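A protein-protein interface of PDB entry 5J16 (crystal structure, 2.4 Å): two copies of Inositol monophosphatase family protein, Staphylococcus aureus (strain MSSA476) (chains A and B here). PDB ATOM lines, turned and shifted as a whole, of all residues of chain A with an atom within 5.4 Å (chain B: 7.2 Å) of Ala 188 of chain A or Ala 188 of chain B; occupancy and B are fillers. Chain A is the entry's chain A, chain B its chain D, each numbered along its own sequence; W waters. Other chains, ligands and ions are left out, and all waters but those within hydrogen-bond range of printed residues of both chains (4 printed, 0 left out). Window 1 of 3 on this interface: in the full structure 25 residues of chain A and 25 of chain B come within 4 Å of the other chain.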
ATOM      1  N   GLY A 161      27.344  -6.726  -1.499  1.00  0.00           N
ATOM      2  CA  GLY A 161      26.635  -5.709  -0.746  1.00  0.00           C
ATOM      3  C   GLY A 161      27.154  -4.359  -1.166  1.00  0.00           C
ATOM      4  O   GLY A 161      28.309  -4.036  -0.913  1.00  0.00           O
ATOM      5  N   ILE A 162      26.308  -3.565  -1.821  1.00  0.00           N
ATOM      6  CA  ILE A 162      26.630  -2.184  -2.109  1.00  0.00           C
ATOM      7  C   ILE A 162      25.429  -1.312  -2.363  1.00  0.00           C
ATOM      8  O   ILE A 162      24.578  -1.614  -3.178  1.00  0.00           O
ATOM      9  CB  ILE A 162      27.554  -2.101  -3.334  1.00  0.00           C
ATOM     10  CG1 ILE A 162      28.104  -0.691  -3.499  1.00  0.00           C
ATOM     11  CG2 ILE A 162      26.872  -2.610  -4.593  1.00  0.00           C
ATOM     12  CD1 ILE A 162      29.094  -0.616  -4.648  1.00  0.00           C
ATOM     13  N   ASN A 163      25.387  -0.174  -1.725  1.00  0.00           N
ATOM     14  CA  ASN A 163      24.262   0.699  -1.890  1.00  0.00           C
ATOM     15  C   ASN A 163      24.224   1.464  -3.237  1.00  0.00           C
ATOM     16  O   ASN A 163      25.249   1.986  -3.698  1.00  0.00           O
ATOM     17  CB  ASN A 163      24.207   1.686  -0.735  1.00  0.00           C
ATOM     18  CG  ASN A 163      22.873   2.371  -0.669  1.00  0.00           C
ATOM     19  OD1 ASN A 163      22.586   3.258  -1.477  1.00  0.00           O
ATOM     20  ND2 ASN A 163      22.014   1.902   0.221  1.00  0.00           N
ATOM     21  N   PRO A 164      23.020   1.578  -3.853  1.00  0.00           N
ATOM     22  CA  PRO A 164      22.866   2.413  -5.034  1.00  0.00           C
ATOM     23  C   PRO A 164      23.450   3.820  -4.906  1.00  0.00           C
ATOM     24  O   PRO A 164      23.890   4.384  -5.894  1.00  0.00           O
ATOM     25  CB  PRO A 164      21.340   2.521  -5.178  1.00  0.00           C
ATOM     26  CG  PRO A 164      20.850   1.255  -4.638  1.00  0.00           C
ATOM     27  CD  PRO A 164      21.740   0.930  -3.502  1.00  0.00           C
ATOM     28  N   ALA A 186      23.549  -7.807  -6.815  1.00  0.00           N
ATOM     29  CA  ALA A 186      23.954  -6.828  -5.800  1.00  0.00           C
ATOM     30  C   ALA A 186      22.820  -6.571  -4.837  1.00  0.00           C
ATOM     31  O   ALA A 186      21.690  -6.568  -5.265  1.00  0.00           O
ATOM     32  CB  ALA A 186      24.356  -5.549  -6.471  1.00  0.00           C
ATOM     33  N   ARG A 187      23.126  -6.370  -3.557  1.00  0.00           N
ATOM     34  CA  ARG A 187      22.108  -6.221  -2.494  1.00  0.00           C
ATOM     35  C   ARG A 187      22.433  -5.004  -1.620  1.00  0.00           C
ATOM     36  O   ARG A 187      23.550  -4.468  -1.678  1.00  0.00           O
ATOM     37  CB  ARG A 187      22.072  -7.478  -1.611  1.00  0.00           C
ATOM     38  CG  ARG A 187      21.738  -8.757  -2.357  1.00  0.00           C
ATOM     39  CD  ARG A 187      20.220  -8.884  -2.583  1.00  0.00           C
ATOM     40  NE  ARG A 187      19.885 -10.148  -3.251  1.00  0.00           N
ATOM     41  CZ  ARG A 187      20.004 -10.368  -4.560  1.00  0.00           C
ATOM     42  NH1 ARG A 187      20.415  -9.428  -5.360  1.00  0.00           N
ATOM     43  NH2 ARG A 187      19.656 -11.541  -5.085  1.00  0.00           N
ATOM     44  N   ALA A 188      21.473  -4.570  -0.819  1.00  0.00           N
ATOM     45  CA  ALA A 188      21.676  -3.390   0.049  1.00  0.00           C
ATOM     46  C   ALA A 188      20.627  -3.377   1.148  1.00  0.00           C
ATOM     47  O   ALA A 188      19.438  -3.263   0.871  1.00  0.00           O
ATOM     48  CB  ALA A 188      21.620  -2.096  -0.750  1.00  0.00           C
ATOM     49  N   TYR A 189      21.099  -3.535   2.386  1.00  0.00           N
ATOM     50  CA  TYR A 189      20.264  -3.772   3.547  1.00  0.00           C
ATOM     51  C   TYR A 189      20.185  -2.582   4.481  1.00  0.00           C
ATOM     52  O   TYR A 189      19.282  -2.518   5.325  1.00  0.00           O
ATOM     53  CB  TYR A 189      20.745  -5.056   4.264  1.00  0.00           C
ATOM     54  CG  TYR A 189      20.727  -6.310   3.340  1.00  0.00           C
ATOM     55  CD1 TYR A 189      19.582  -6.662   2.634  1.00  0.00           C
ATOM     56  CD2 TYR A 189      21.833  -7.137   3.215  1.00  0.00           C
ATOM     57  CE1 TYR A 189      19.548  -7.781   1.823  1.00  0.00           C
ATOM     58  CE2 TYR A 189      21.808  -8.255   2.408  1.00  0.00           C
ATOM     59  CZ  TYR A 189      20.659  -8.571   1.712  1.00  0.00           C
ATOM     60  OH  TYR A 189      20.606  -9.686   0.903  1.00  0.00           O
ATOM     61  N   GLY A 190      21.072  -1.609   4.341  1.00  0.00           N
ATOM     62  CA  GLY A 190      21.016  -0.442   5.216  1.00  0.00           C
ATOM     63  C   GLY A 190      21.529  -0.645   6.638  1.00  0.00           C
ATOM     64  O   GLY A 190      21.147   0.122   7.558  1.00  0.00           O
ATOM     65  N   GLU A 195      25.470  -6.133   7.400  1.00  0.00           N
ATOM     66  CA  GLU A 195      26.089  -6.544   6.147  1.00  0.00           C
ATOM     67  C   GLU A 195      27.470  -7.164   6.240  1.00  0.00           C
ATOM     68  O   GLU A 195      27.811  -8.046   5.455  1.00  0.00           O
ATOM     69  CB  GLU A 195      26.087  -5.392   5.160  1.00  0.00           C
ATOM     70  CG  GLU A 195      24.682  -5.218   4.648  1.00  0.00           C
ATOM     71  CD  GLU A 195      24.522  -4.029   3.805  1.00  0.00           C
ATOM     72  OE1 GLU A 195      24.215  -2.967   4.369  1.00  0.00           O
ATOM     73  OE2 GLU A 195      24.726  -4.180   2.597  1.00  0.00           O
ATOM     74  N   ILE B 160      13.707   3.678  -0.821  1.00  0.00           N
ATOM     75  CA  ILE B 160      13.297   3.077  -2.092  1.00  0.00           C
ATOM     76  C   ILE B 160      14.030   1.769  -2.441  1.00  0.00           C
ATOM     77  O   ILE B 160      15.216   1.585  -2.137  1.00  0.00           O
ATOM     78  CB  ILE B 160      13.454   4.057  -3.260  1.00  0.00           C
ATOM     79  CG1 ILE B 160      14.899   4.447  -3.496  1.00  0.00           C
ATOM     80  CG2 ILE B 160      12.636   5.302  -2.983  1.00  0.00           C
ATOM     81  CD1 ILE B 160      15.061   5.224  -4.802  1.00  0.00           C
ATOM     82  N   GLY B 161      13.291   0.887  -3.101  1.00  0.00           N
ATOM     83  CA  GLY B 161      13.817  -0.349  -3.586  1.00  0.00           C
ATOM     84  C   GLY B 161      14.262  -0.128  -5.000  1.00  0.00           C
ATOM     85  O   GLY B 161      13.424   0.068  -5.877  1.00  0.00           O
ATOM     86  N   ILE B 162      15.575  -0.122  -5.215  1.00  0.00           N
ATOM     87  CA  ILE B 162      16.137  -0.156  -6.558  1.00  0.00           C
ATOM     88  C   ILE B 162      17.488  -0.891  -6.606  1.00  0.00           C
ATOM     89  O   ILE B 162      18.381  -0.641  -5.799  1.00  0.00           O
ATOM     90  CB  ILE B 162      16.193   1.244  -7.188  1.00  0.00           C
ATOM     91  CG1 ILE B 162      16.926   1.184  -8.529  1.00  0.00           C
ATOM     92  CG2 ILE B 162      16.824   2.271  -6.260  1.00  0.00           C
ATOM     93  CD1 ILE B 162      16.677   2.406  -9.391  1.00  0.00           C
ATOM     94  N   ASN B 163      17.624  -1.823  -7.545  1.00  0.00           N
ATOM     95  CA  ASN B 163      18.834  -2.586  -7.620  1.00  0.00           C
ATOM     96  C   ASN B 163      19.990  -1.759  -8.214  1.00  0.00           C
ATOM     97  O   ASN B 163      19.797  -1.024  -9.204  1.00  0.00           O
ATOM     98  CB  ASN B 163      18.656  -3.850  -8.430  1.00  0.00           C
ATOM     99  CG  ASN B 163      19.761  -4.862  -8.145  1.00  0.00           C
ATOM    100  OD1 ASN B 163      20.872  -4.729  -8.653  1.00  0.00           O
ATOM    101  ND2 ASN B 163      19.474  -5.841  -7.290  1.00  0.00           N
ATOM    102  N   PRO B 164      21.193  -1.889  -7.626  1.00  0.00           N
ATOM    103  CA  PRO B 164      22.350  -1.229  -8.173  1.00  0.00           C
ATOM    104  C   PRO B 164      22.600  -1.528  -9.640  1.00  0.00           C
ATOM    105  O   PRO B 164      23.109  -0.665 -10.334  1.00  0.00           O
ATOM    106  CB  PRO B 164      23.501  -1.787  -7.331  1.00  0.00           C
ATOM    107  CG  PRO B 164      22.882  -2.065  -6.026  1.00  0.00           C
ATOM    108  CD  PRO B 164      21.523  -2.590  -6.368  1.00  0.00           C
ATOM    109  N   ALA B 186      18.258   3.977  -0.271  1.00  0.00           N
ATOM    110  CA  ALA B 186      17.785   2.934  -1.175  1.00  0.00           C
ATOM    111  C   ALA B 186      18.179   1.587  -0.616  1.00  0.00           C
ATOM    112  O   ALA B 186      19.079   1.499   0.228  1.00  0.00           O
ATOM    113  CB  ALA B 186      18.359   3.091  -2.561  1.00  0.00           C
ATOM    114  N   ARG B 187      17.473   0.567  -1.096  1.00  0.00           N
ATOM    115  CA  ARG B 187      17.617  -0.793  -0.661  1.00  0.00           C
ATOM    116  C   ARG B 187      17.425  -1.781  -1.817  1.00  0.00           C
ATOM    117  O   ARG B 187      16.773  -1.466  -2.793  1.00  0.00           O
ATOM    118  CB  ARG B 187      16.552  -1.094   0.376  1.00  0.00           C
ATOM    119  CG  ARG B 187      16.601  -0.241   1.622  1.00  0.00           C
ATOM    120  CD  ARG B 187      17.681  -0.742   2.572  1.00  0.00           C
ATOM    121  NE  ARG B 187      17.670   0.072   3.792  1.00  0.00           N
ATOM    122  CZ  ARG B 187      18.301   1.225   3.931  1.00  0.00           C
ATOM    123  NH1 ARG B 187      19.048   1.721   2.959  1.00  0.00           N
ATOM    124  NH2 ARG B 187      18.239   1.855   5.078  1.00  0.00           N
ATOM    125  N   ALA B 188      17.949  -2.999  -1.684  1.00  0.00           N
ATOM    126  CA  ALA B 188      17.765  -4.003  -2.715  1.00  0.00           C
ATOM    127  C   ALA B 188      17.849  -5.362  -2.065  1.00  0.00           C
ATOM    128  O   ALA B 188      18.892  -5.734  -1.493  1.00  0.00           O
ATOM    129  CB  ALA B 188      18.806  -3.850  -3.816  1.00  0.00           C
ATOM    130  N   TYR B 189      16.735  -6.086  -2.160  1.00  0.00           N
ATOM    131  CA  TYR B 189      16.555  -7.335  -1.475  1.00  0.00           C
ATOM    132  C   TYR B 189      16.636  -8.549  -2.396  1.00  0.00           C
ATOM    133  O   TYR B 189      16.813  -9.645  -1.900  1.00  0.00           O
ATOM    134  CB  TYR B 189      15.254  -7.320  -0.696  1.00  0.00           C
ATOM    135  CG  TYR B 189      15.092  -6.194   0.321  1.00  0.00           C
ATOM    136  CD1 TYR B 189      16.167  -5.676   1.058  1.00  0.00           C
ATOM    137  CD2 TYR B 189      13.829  -5.659   0.573  1.00  0.00           C
ATOM    138  CE1 TYR B 189      15.984  -4.665   2.018  1.00  0.00           C
ATOM    139  CE2 TYR B 189      13.647  -4.641   1.501  1.00  0.00           C
ATOM    140  CZ  TYR B 189      14.726  -4.162   2.224  1.00  0.00           C
ATOM    141  OH  TYR B 189      14.470  -3.178   3.130  1.00  0.00           O
ATOM    142  N   GLY B 190      16.525  -8.349  -3.710  1.00  0.00           N
ATOM    143  CA  GLY B 190      16.633  -9.438  -4.691  1.00  0.00           C
ATOM    144  C   GLY B 190      15.416 -10.332  -4.952  1.00  0.00           C
ATOM    145  O   GLY B 190      15.573 -11.472  -5.412  1.00  0.00           O
ATOM    146  N   SER B 191      14.214  -9.831  -4.662  1.00  0.00           N
ATOM    147  CA  SER B 191      12.961 -10.573  -4.969  1.00  0.00           C
ATOM    148  C   SER B 191      11.876  -9.567  -5.202  1.00  0.00           C
ATOM    149  O   SER B 191      11.372  -8.988  -4.257  1.00  0.00           O
ATOM    150  CB  SER B 191      12.506 -11.476  -3.820  1.00  0.00           C
ATOM    151  OG  SER B 191      11.089 -11.724  -3.882  1.00  0.00           O
ATOM    152  N   GLU B 195       9.700  -7.452  -2.590  1.00  0.00           N
ATOM    153  CA  GLU B 195       9.872  -5.995  -2.556  1.00  0.00           C
ATOM    154  C   GLU B 195       8.565  -5.244  -2.817  1.00  0.00           C
ATOM    155  O   GLU B 195       8.315  -4.190  -2.208  1.00  0.00           O
ATOM    156  CB  GLU B 195      11.000  -5.546  -3.476  1.00  0.00           C
ATOM    157  CG  GLU B 195      12.351  -5.935  -2.899  1.00  0.00           C
ATOM    158  CD  GLU B 195      13.534  -5.461  -3.713  1.00  0.00           C
ATOM    159  OE1 GLU B 195      14.201  -6.297  -4.370  1.00  0.00           O
ATOM    160  OE2 GLU B 195      13.796  -4.232  -3.689  1.00  0.00           O
ATOM    161  N   LEU B 204       9.255  -0.530   2.571  1.00  0.00           N
ATOM    162  CA  LEU B 204       9.781   0.355   1.559  1.00  0.00           C
ATOM    163  C   LEU B 204       8.634   1.297   1.236  1.00  0.00           C
ATOM    164  O   LEU B 204       7.482   0.892   1.292  1.00  0.00           O
ATOM    165  CB  LEU B 204      10.238  -0.430   0.304  1.00  0.00           C
ATOM    166  CG  LEU B 204      11.463  -1.344   0.433  1.00  0.00           C
ATOM    167  CD1 LEU B 204      11.603  -2.209  -0.804  1.00  0.00           C
ATOM    168  CD2 LEU B 204      12.769  -0.596   0.684  1.00  0.00           C
ATOM    169  N   TYR B 207       9.193   1.031  -4.845  1.00  0.00           N
ATOM    170  CA  TYR B 207      10.062   0.052  -5.500  1.00  0.00           C
ATOM    171  C   TYR B 207       9.955   0.233  -7.003  1.00  0.00           C
ATOM    172  O   TYR B 207       8.879   0.553  -7.517  1.00  0.00           O
ATOM    173  CB  TYR B 207       9.662  -1.377  -5.094  1.00  0.00           C
ATOM    174  CG  TYR B 207      10.124  -2.460  -5.999  1.00  0.00           C
ATOM    175  CD1 TYR B 207      11.441  -2.863  -6.001  1.00  0.00           C
ATOM    176  CD2 TYR B 207       9.241  -3.115  -6.844  1.00  0.00           C
ATOM    177  CE1 TYR B 207      11.892  -3.887  -6.840  1.00  0.00           C
ATOM    178  CE2 TYR B 207       9.678  -4.135  -7.692  1.00  0.00           C
ATOM    179  CZ  TYR B 207      11.013  -4.497  -7.691  1.00  0.00           C
ATOM    180  OH  TYR B 207      11.466  -5.493  -8.501  1.00  0.00           O
HETATM  181  O   HOH W   1      16.881  -3.578   5.175  1.00  0.00           O
HETATM  182  O   HOH W   2      17.310 -13.297  -5.779  1.00  0.00           O
HETATM  183  O   HOH W   3      19.217   2.004   7.860  1.00  0.00           O
HETATM  184  O   HOH W   4      17.984 -10.392   0.291  1.00  0.00           O
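Printed residues of chain B within 4 Å of Ala 188 of chain A: Arg 187 (3.4 Å), Ala 188 (2.9 Å) and Tyr 189 (3.9 Å). Ala 188 of chain B touches just these residues of chain A: Arg 187 (3.4 Å), Ala 188 (2.9 Å) and Tyr 189 (3.95 Å). Of the printed residues of chain B, Ile 162 of chain A touches Pro 164. Of the printed residues of chain A, Ala 186 of chain B touches Asn 163 and Pro 164. Of the printed residues of chain A, Tyr 189 of chain B touches Arg 187 (3.4 Å), Ala 188 (3.9 Å) and Tyr 189 (3.9 Å). Gly 161 of chain A touches none of the printed residues of chain B. The nearest residue of chain B that does not touch Ala 188 of chain A is Ala 186 of chain B (4.5 Å). The nearest residue of chain A that does not touch Ala 188 of chain B is Ala 186 of chain A (4.2 Å).
N of Ile 162 of chain A lies within hydrogen-bond range of O of Arg 187 of chain A, 2.9 Å away. N of Gly 190 of chain A is in hydrogen-bond range of OE1 of Glu 195 of chain A, 3.4 Å away. O of Ile 160 of chain B sits at hydrogen-bond distance from N of Arg 187 of chain B, 2.7 Å away. N of Ile 162 of chain B is in hydrogen-bond range of O of Arg 187 of chain B, 3.0 Å away. The backbone NH of Tyr 189 of chain B sits at hydrogen-bond distance from the side-chain carboxylate of Glu 195 of chain B, at 3.4 Å. The backbone NH (N) of Gly 190 of chain B sits at hydrogen-bond distance from the side-chain carboxylate (OE1) of Glu 195 of chain B, 3.2 Å away.
Ile 162 of chain A touches Pro 164 of chain B (O to CG, 3.3 Å). Pro 164 of chain A touches Ile 162 of chain B (CG to O, 3.3 Å). Pro 164 of chain A touches Ala 186 of chain B. CB of Ala 186 of chain A touches CG of Pro 164 of chain B (3.8 Å). Arg 187 of chain A touches Ala 188 of chain B (CA to O, 3.4 Å). Arg 187 of chain A touches Gly 190 of chain B. Arg 187 of chain B touches Ala 188 of chain A. Tyr 189 of chain B touches Ala 188 of chain A (CE1 to O, 3.9 Å). CE1 of Tyr 189 of chain A touches O of Ala 188 of chain B, at 3.95 Å. Tyr 189 of chain B touches Tyr 189 of chain A (CD1 to CD1, 3.9 Å).
Hydrophobic or aromatic side chains of chain A within 4 Å of the printed part of chain B: Pro 164, Ala 186, Ala 188 and Tyr 189. Along chain A the printed residues that touch a printed residue of chain B span positions 162 to 190. Along chain B the printed residues that touch a printed residue of chain A span positions 162 to 190. Among the printed residues, 16 pairs touch across the chains. Among the printed residues, no Asp or Glu carboxylate lies within 4 Å of a Lys or Arg side-chain nitrogen of the other chain.
Water W2 lies within hydrogen-bond range of O of Gly 190 of chain B and NH2 of Arg 187 of chain A. Water W4 lies within hydrogen-bond range of the backbone carbonyl oxygen (O) of Tyr 189 of chain B (2.6 Å) and the side-chain hydroxyl (OH) of Tyr 189 of chain A (2.8 Å). Water W1 lies within hydrogen-bond range of the backbone carbonyl oxygen (O) of Tyr 189 of chain A and the side-chain hydroxyl (OH) of Tyr 189 of chain B. Water W3 bridges the backbone carbonyl oxygen of Gly 190 of chain A (2.7 Å) and the guanidinium group of Arg 187 of chain B (3.0 Å).
Ile 162 of chain A touches Pro 164 of chain B, and with the chains exchanged Pro 164 of chain A touches Ile 162 of chain B. Arg 187 of chain A touches Tyr 189 of chain B, and with the chains exchanged Tyr 189 of chain A touches Arg 187 of chain B. Arg 187 of chain A touches Gly 190 of chain B, and with the chains exchanged Gly 190 of chain A touches Arg 187 of chain B. Ala 188 of chain B touches its own counterpart, Ala 188 of chain A. Positions printed for both chains: 161, 162, 163, 164, 186, 187, 188, 189, 190 and 195. Of the 16 pairs that touch across the chains among the printed residues, 16 have their exchanged pair printed and touching as well.
The side-chain amide nitrogen of Asn 163 of chain A is in hydrogen-bond range of the backbone carbonyl oxygen of Ala 186 of chain B, 3.0 Å away. The backbone carbonyl oxygen (O) of Ala 186 of chain A lies within hydrogen-bond range of the side-chain amide nitrogen (ND2) of Asn 163 of chain B (3.1 Å). O of Tyr 189 of chain B sits at hydrogen-bond distance from NE of Arg 187 of chain A. The backbone carbonyl oxygen of Ala 188 of chain B sits at hydrogen-bond distance from the backbone NH of Ala 188 of chain A (2.9 Å). The backbone carbonyl oxygen of Tyr 189 of chain A sits at hydrogen-bond distance from the guanidinium group of Arg 187 of chain B (3.4 Å).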
